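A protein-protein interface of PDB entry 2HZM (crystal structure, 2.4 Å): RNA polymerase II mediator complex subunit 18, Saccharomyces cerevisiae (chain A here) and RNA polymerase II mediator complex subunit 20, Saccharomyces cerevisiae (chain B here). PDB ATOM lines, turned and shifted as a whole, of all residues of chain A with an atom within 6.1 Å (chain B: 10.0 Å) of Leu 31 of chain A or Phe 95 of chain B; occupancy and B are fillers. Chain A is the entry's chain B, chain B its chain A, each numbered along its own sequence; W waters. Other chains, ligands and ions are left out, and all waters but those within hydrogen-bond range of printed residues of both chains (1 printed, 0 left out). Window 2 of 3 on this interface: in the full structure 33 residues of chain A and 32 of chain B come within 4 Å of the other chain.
NZ of Lys 220 of chain A is in hydrogen-bond range of O of Phe 95 of chain B (2.6 Å).
The backbone carbonyl oxygen (O) of Asn 34 of chain A lies within hydrogen-bond range of the side-chain amide nitrogen (ND2) of Asn 96 of chain B, 2.8 Å away.
O of Leu 31 of chain A lies within hydrogen-bond range of N of Lys 220 of chain A (2.7 Å).
O of Ala 92 of chain B lies close to OD1 of Asn 96 of chain B.
O of Leu 93 of chain B lies close to OD1 of Asn 96 of chain B.
The backbone carbonyl oxygen of Gly 218 of chain A lies within hydrogen-bond range of the backbone NH of Tyr 33 of chain A.
The backbone NH of Ser 98 of chain B is in hydrogen-bond range of the side-chain amide oxygen of Asn 96 of chain B, 2.8 Å away.
CB of Leu 31 of chain A touches CE1 of Phe 95 of chain B, 3.9 Å away.
Leu 32 of chain A touches Phe 95 of chain B.
CB of Tyr 33 of chain A touches CE2 of Phe 95 of chain B (3.6 Å).
Tyr 33 of chain A touches Asn 96 of chain B (CD1 to O, 3.5 Å).
Leu 31 of chain A touches just one residue of chain B: Phe 95.
No residue of chain B comes within 4 Å of Pro 30 of chain A.
Of chain B, only Phe 95 comes within 4 Å of Leu 32 of chain A.
Of chain B, only Phe 95 (2.6 Å) comes within 4 Å of Lys 220 of chain A.
Of the printed residues of chain B, Tyr 33 of chain A touches Phe 95 (3.6 Å) and Asn 96 (3.5 Å).
Of the printed residues of chain B, Asn 34 of chain A touches Asn 96 (2.8 Å).
Phe 221 of chain A touches none of the printed residues of chain B.
Of the 13 printed residues of chain B, 2 touch a printed residue of chain A.
Printed residues of chain B that touch a printed residue of chain A: Phe 95 and Asn 96.
Hydrophobic or aromatic side chains of chain B within 4 Å of the printed part of chain A: Phe 95.
Among the printed residues, 6 pairs touch across the chains.
Among the printed residues, no Asp or Glu carboxylate lies within 4 Å of a Lys or Arg side-chain nitrogen of the other chain.
Water W1 bridges NZ of Lys 220 of chain A (2.9 Å) and O of Val 94 of chain B (3.4 Å).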
ATOM      1  N   PRO A  29      -9.422  25.046  36.129  1.00  0.00           N
ATOM      2  CA  PRO A  29      -9.149  26.001  35.050  1.00  0.00           C
ATOM      3  C   PRO A  29      -9.103  25.348  33.677  1.00  0.00           C
ATOM      4  O   PRO A  29      -8.865  24.150  33.559  1.00  0.00           O
ATOM      5  CB  PRO A  29      -7.782  26.548  35.426  1.00  0.00           C
ATOM      6  CG  PRO A  29      -7.085  25.289  35.905  1.00  0.00           C
ATOM      7  CD  PRO A  29      -8.167  24.681  36.825  1.00  0.00           C
ATOM      8  N   PRO A  30      -9.336  26.144  32.624  1.00  0.00           N
ATOM      9  CA  PRO A  30      -9.306  25.642  31.252  1.00  0.00           C
ATOM     10  C   PRO A  30      -7.837  25.529  30.847  1.00  0.00           C
ATOM     11  O   PRO A  30      -7.093  26.508  30.930  1.00  0.00           O
ATOM     12  CB  PRO A  30     -10.060  26.721  30.470  1.00  0.00           C
ATOM     13  CG  PRO A  30      -9.812  28.002  31.272  1.00  0.00           C
ATOM     14  CD  PRO A  30      -9.895  27.514  32.697  1.00  0.00           C
ATOM     15  N   LEU A  31      -7.413  24.344  30.418  1.00  0.00           N
ATOM     16  CA  LEU A  31      -6.020  24.147  30.037  1.00  0.00           C
ATOM     17  C   LEU A  31      -5.837  24.089  28.533  1.00  0.00           C
ATOM     18  O   LEU A  31      -6.342  23.194  27.857  1.00  0.00           O
ATOM     19  CB  LEU A  31      -5.479  22.870  30.674  1.00  0.00           C
ATOM     20  CG  LEU A  31      -5.635  22.774  32.192  1.00  0.00           C
ATOM     21  CD1 LEU A  31      -5.275  21.390  32.663  1.00  0.00           C
ATOM     22  CD2 LEU A  31      -4.765  23.826  32.866  1.00  0.00           C
ATOM     23  N   LEU A  32      -5.088  25.048  28.028  1.00  0.00           N
ATOM     24  CA  LEU A  32      -4.797  25.201  26.609  1.00  0.00           C
ATOM     25  C   LEU A  32      -3.947  24.047  26.057  1.00  0.00           C
ATOM     26  O   LEU A  32      -2.972  23.617  26.687  1.00  0.00           O
ATOM     27  CB  LEU A  32      -4.056  26.518  26.449  1.00  0.00           C
ATOM     28  CG  LEU A  32      -4.082  27.453  25.253  1.00  0.00           C
ATOM     29  CD1 LEU A  32      -5.473  27.636  24.669  1.00  0.00           C
ATOM     30  CD2 LEU A  32      -3.542  28.794  25.780  1.00  0.00           C
ATOM     31  N   TYR A  33      -4.305  23.569  24.870  1.00  0.00           N
ATOM     32  CA  TYR A  33      -3.578  22.484  24.237  1.00  0.00           C
ATOM     33  C   TYR A  33      -3.851  22.517  22.741  1.00  0.00           C
ATOM     34  O   TYR A  33      -4.783  23.180  22.283  1.00  0.00           O
ATOM     35  CB  TYR A  33      -4.082  21.150  24.791  1.00  0.00           C
ATOM     36  CG  TYR A  33      -5.395  20.735  24.162  1.00  0.00           C
ATOM     37  CD1 TYR A  33      -5.415  19.959  22.998  1.00  0.00           C
ATOM     38  CD2 TYR A  33      -6.618  21.189  24.681  1.00  0.00           C
ATOM     39  CE1 TYR A  33      -6.606  19.640  22.368  1.00  0.00           C
ATOM     40  CE2 TYR A  33      -7.825  20.887  24.053  1.00  0.00           C
ATOM     41  CZ  TYR A  33      -7.814  20.108  22.898  1.00  0.00           C
ATOM     42  OH  TYR A  33      -8.995  19.772  22.272  1.00  0.00           O
ATOM     43  N   ASN A  34      -3.044  21.791  21.975  1.00  0.00           N
ATOM     44  CA  ASN A  34      -3.260  21.700  20.528  1.00  0.00           C
ATOM     45  C   ASN A  34      -2.765  20.344  20.055  1.00  0.00           C
ATOM     46  O   ASN A  34      -2.008  19.682  20.750  1.00  0.00           O
ATOM     47  CB  ASN A  34      -2.505  22.808  19.779  1.00  0.00           C
ATOM     48  CG  ASN A  34      -0.984  22.594  19.773  1.00  0.00           C
ATOM     49  OD1 ASN A  34      -0.464  21.693  19.102  1.00  0.00           O
ATOM     50  ND2 ASN A  34      -0.270  23.434  20.517  1.00  0.00           N
ATOM     51  N   GLY A 218      -7.475  24.204  21.464  1.00  0.00           N
ATOM     52  CA  GLY A 218      -8.574  24.332  22.398  1.00  0.00           C
ATOM     53  C   GLY A 218      -8.135  24.377  23.847  1.00  0.00           C
ATOM     54  O   GLY A 218      -6.970  24.651  24.160  1.00  0.00           O
ATOM     55  N   VAL A 219      -9.091  24.158  24.737  1.00  0.00           N
ATOM     56  CA  VAL A 219      -8.810  24.121  26.160  1.00  0.00           C
ATOM     57  C   VAL A 219      -9.487  22.869  26.671  1.00  0.00           C
ATOM     58  O   VAL A 219     -10.521  22.447  26.142  1.00  0.00           O
ATOM     59  CB  VAL A 219      -9.362  25.372  26.930  1.00  0.00           C
ATOM     60  CG1 VAL A 219      -8.503  26.586  26.618  1.00  0.00           C
ATOM     61  CG2 VAL A 219     -10.814  25.634  26.569  1.00  0.00           C
ATOM     62  N   LYS A 220      -8.900  22.241  27.669  1.00  0.00           N
ATOM     63  CA  LYS A 220      -9.525  21.041  28.189  1.00  0.00           C
ATOM     64  C   LYS A 220      -9.745  21.185  29.674  1.00  0.00           C
ATOM     65  O   LYS A 220      -9.078  21.974  30.338  1.00  0.00           O
ATOM     66  CB  LYS A 220      -8.661  19.797  27.896  1.00  0.00           C
ATOM     67  CG  LYS A 220      -7.324  19.813  28.593  1.00  0.00           C
ATOM     68  CD  LYS A 220      -6.917  18.413  29.074  1.00  0.00           C
ATOM     69  CE  LYS A 220      -6.599  17.487  27.930  1.00  0.00           C
ATOM     70  NZ  LYS A 220      -6.084  16.158  28.383  1.00  0.00           N
ATOM     71  N   PHE A 221     -10.707  20.435  30.184  1.00  0.00           N
ATOM     72  CA  PHE A 221     -10.984  20.441  31.602  1.00  0.00           C
ATOM     73  C   PHE A 221     -10.962  19.014  32.101  1.00  0.00           C
ATOM     74  O   PHE A 221     -11.449  18.094  31.433  1.00  0.00           O
ATOM     75  CB  PHE A 221     -12.369  21.021  31.919  1.00  0.00           C
ATOM     76  CG  PHE A 221     -12.571  22.433  31.447  1.00  0.00           C
ATOM     77  CD1 PHE A 221     -12.740  22.710  30.094  1.00  0.00           C
ATOM     78  CD2 PHE A 221     -12.631  23.477  32.358  1.00  0.00           C
ATOM     79  CE1 PHE A 221     -12.973  24.009  29.647  1.00  0.00           C
ATOM     80  CE2 PHE A 221     -12.867  24.785  31.926  1.00  0.00           C
ATOM     81  CZ  PHE A 221     -13.038  25.050  30.569  1.00  0.00           C
ATOM     82  N   PHE A 222     -10.383  18.836  33.275  1.00  0.00           N
ATOM     83  CA  PHE A 222     -10.360  17.542  33.907  1.00  0.00           C
ATOM     84  C   PHE A 222     -11.539  17.513  34.865  1.00  0.00           C
ATOM     85  O   PHE A 222     -11.707  18.417  35.677  1.00  0.00           O
ATOM     86  CB  PHE A 222      -9.058  17.353  34.679  1.00  0.00           C
ATOM     87  CG  PHE A 222      -7.887  17.067  33.800  1.00  0.00           C
ATOM     88  CD1 PHE A 222      -7.875  15.933  32.992  1.00  0.00           C
ATOM     89  CD2 PHE A 222      -6.793  17.928  33.765  1.00  0.00           C
ATOM     90  CE1 PHE A 222      -6.790  15.664  32.167  1.00  0.00           C
ATOM     91  CE2 PHE A 222      -5.701  17.664  32.938  1.00  0.00           C
ATOM     92  CZ  PHE A 222      -5.698  16.534  32.140  1.00  0.00           C
ATOM     93  N   ILE B  89       6.557   7.256  27.260  1.00  0.00           N
ATOM     94  CA  ILE B  89       5.596   8.141  26.627  1.00  0.00           C
ATOM     95  C   ILE B  89       5.844   9.610  26.953  1.00  0.00           C
ATOM     96  O   ILE B  89       5.835   9.990  28.113  1.00  0.00           O
ATOM     97  CB  ILE B  89       4.138   7.781  27.056  1.00  0.00           C
ATOM     98  CG1 ILE B  89       3.802   6.347  26.641  1.00  0.00           C
ATOM     99  CG2 ILE B  89       3.143   8.714  26.378  1.00  0.00           C
ATOM    100  CD1 ILE B  89       2.443   5.862  27.127  1.00  0.00           C
ATOM    101  N   PRO B  90       6.074  10.455  25.931  1.00  0.00           N
ATOM    102  CA  PRO B  90       6.304  11.888  26.205  1.00  0.00           C
ATOM    103  C   PRO B  90       5.069  12.436  26.927  1.00  0.00           C
ATOM    104  O   PRO B  90       3.947  12.322  26.431  1.00  0.00           O
ATOM    105  CB  PRO B  90       6.442  12.500  24.817  1.00  0.00           C
ATOM    106  CG  PRO B  90       6.964  11.324  23.971  1.00  0.00           C
ATOM    107  CD  PRO B  90       6.133  10.170  24.481  1.00  0.00           C
ATOM    108  N   PRO B  91       5.260  13.016  28.116  1.00  0.00           N
ATOM    109  CA  PRO B  91       4.137  13.572  28.894  1.00  0.00           C
ATOM    110  C   PRO B  91       3.271  14.575  28.122  1.00  0.00           C
ATOM    111  O   PRO B  91       2.067  14.699  28.374  1.00  0.00           O
ATOM    112  CB  PRO B  91       4.829  14.223  30.103  1.00  0.00           C
ATOM    113  CG  PRO B  91       6.078  13.356  30.278  1.00  0.00           C
ATOM    114  CD  PRO B  91       6.542  13.153  28.832  1.00  0.00           C
ATOM    115  N   ALA B  92       3.879  15.284  27.184  1.00  0.00           N
ATOM    116  CA  ALA B  92       3.156  16.285  26.408  1.00  0.00           C
ATOM    117  C   ALA B  92       2.093  15.626  25.541  1.00  0.00           C
ATOM    118  O   ALA B  92       1.000  16.186  25.344  1.00  0.00           O
ATOM    119  CB  ALA B  92       4.140  17.087  25.529  1.00  0.00           C
ATOM    120  N   LEU B  93       2.424  14.442  25.024  1.00  0.00           N
ATOM    121  CA  LEU B  93       1.527  13.680  24.155  1.00  0.00           C
ATOM    122  C   LEU B  93       0.271  13.236  24.863  1.00  0.00           C
ATOM    123  O   LEU B  93      -0.791  13.108  24.253  1.00  0.00           O
ATOM    124  CB  LEU B  93       2.242  12.442  23.610  1.00  0.00           C
ATOM    125  CG  LEU B  93       2.444  12.403  22.106  1.00  0.00           C
ATOM    126  CD1 LEU B  93       2.833  13.791  21.614  1.00  0.00           C
ATOM    127  CD2 LEU B  93       3.487  11.343  21.741  1.00  0.00           C
ATOM    128  N   VAL B  94       0.406  12.956  26.149  1.00  0.00           N
ATOM    129  CA  VAL B  94      -0.724  12.521  26.947  1.00  0.00           C
ATOM    130  C   VAL B  94      -1.578  13.720  27.342  1.00  0.00           C
ATOM    131  O   VAL B  94      -2.807  13.673  27.219  1.00  0.00           O
ATOM    132  CB  VAL B  94      -0.267  11.809  28.244  1.00  0.00           C
ATOM    133  CG1 VAL B  94      -1.485  11.505  29.127  1.00  0.00           C
ATOM    134  CG2 VAL B  94       0.462  10.511  27.894  1.00  0.00           C
ATOM    135  N   PHE B  95      -0.936  14.790  27.812  1.00  0.00           N
ATOM    136  CA  PHE B  95      -1.693  15.979  28.210  1.00  0.00           C
ATOM    137  C   PHE B  95      -2.595  16.531  27.090  1.00  0.00           C
ATOM    138  O   PHE B  95      -3.755  16.844  27.328  1.00  0.00           O
ATOM    139  CB  PHE B  95      -0.765  17.112  28.690  1.00  0.00           C
ATOM    140  CG  PHE B  95      -1.443  18.471  28.697  1.00  0.00           C
ATOM    141  CD1 PHE B  95      -2.405  18.781  29.663  1.00  0.00           C
ATOM    142  CD2 PHE B  95      -1.194  19.393  27.679  1.00  0.00           C
ATOM    143  CE1 PHE B  95      -3.114  19.981  29.616  1.00  0.00           C
ATOM    144  CE2 PHE B  95      -1.901  20.607  27.614  1.00  0.00           C
ATOM    145  CZ  PHE B  95      -2.860  20.901  28.576  1.00  0.00           C
ATOM    146  N   ASN B  96      -2.064  16.630  25.876  1.00  0.00           N
ATOM    147  CA  ASN B  96      -2.802  17.192  24.753  1.00  0.00           C
ATOM    148  C   ASN B  96      -3.776  16.224  24.093  1.00  0.00           C
ATOM    149  O   ASN B  96      -4.479  16.614  23.142  1.00  0.00           O
ATOM    150  CB  ASN B  96      -1.825  17.698  23.690  1.00  0.00           C
ATOM    151  CG  ASN B  96      -1.501  16.635  22.668  1.00  0.00           C
ATOM    152  OD1 ASN B  96      -1.279  15.473  23.028  1.00  0.00           O
ATOM    153  ND2 ASN B  96      -1.477  17.015  21.385  1.00  0.00           N
ATOM    154  N   GLY B  97      -3.795  14.971  24.552  1.00  0.00           N
ATOM    155  CA  GLY B  97      -4.722  14.017  23.977  1.00  0.00           C
ATOM    156  C   GLY B  97      -4.311  13.294  22.697  1.00  0.00           C
ATOM    157  O   GLY B  97      -5.119  12.565  22.115  1.00  0.00           O
ATOM    158  N   SER B  98      -3.074  13.493  22.246  1.00  0.00           N
ATOM    159  CA  SER B  98      -2.592  12.811  21.053  1.00  0.00           C
ATOM    160  C   SER B  98      -2.571  11.328  21.389  1.00  0.00           C
ATOM    161  O   SER B  98      -2.944  10.491  20.575  1.00  0.00           O
ATOM    162  CB  SER B  98      -1.191  13.287  20.681  1.00  0.00           C
ATOM    163  OG  SER B  98      -1.259  14.517  19.998  1.00  0.00           O
ATOM    164  N   SER B  99      -2.167  11.022  22.616  1.00  0.00           N
ATOM    165  CA  SER B  99      -2.115   9.653  23.105  1.00  0.00           C
ATOM    166  C   SER B  99      -3.167   9.438  24.191  1.00  0.00           C
ATOM    167  O   SER B  99      -3.494  10.347  24.953  1.00  0.00           O
ATOM    168  CB  SER B  99      -0.726   9.367  23.687  1.00  0.00           C
ATOM    169  OG  SER B  99      -0.728   8.230  24.539  1.00  0.00           O
ATOM    170  N   THR B 100      -3.700   8.228  24.257  1.00  0.00           N
ATOM    171  CA  THR B 100      -4.687   7.877  25.263  1.00  0.00           C
ATOM    172  C   THR B 100      -3.905   7.620  26.532  1.00  0.00           C
ATOM    173  O   THR B 100      -4.465   7.560  27.620  1.00  0.00           O
ATOM    174  CB  THR B 100      -5.384   6.547  24.909  1.00  0.00           C
ATOM    175  OG1 THR B 100      -4.381   5.537  24.683  1.00  0.00           O
ATOM    176  CG2 THR B 100      -6.235   6.697  23.670  1.00  0.00           C
ATOM    177  N   GLY B 101      -2.598   7.446  26.378  1.00  0.00           N
ATOM    178  CA  GLY B 101      -1.761   7.142  27.520  1.00  0.00           C
ATOM    179  C   GLY B 101      -1.809   5.643  27.786  1.00  0.00           C
ATOM    180  O   GLY B 101      -1.220   5.156  28.754  1.00  0.00           O
HETATM  181  O   HOH W   1      -5.093  13.886  29.791  1.00  0.00           O
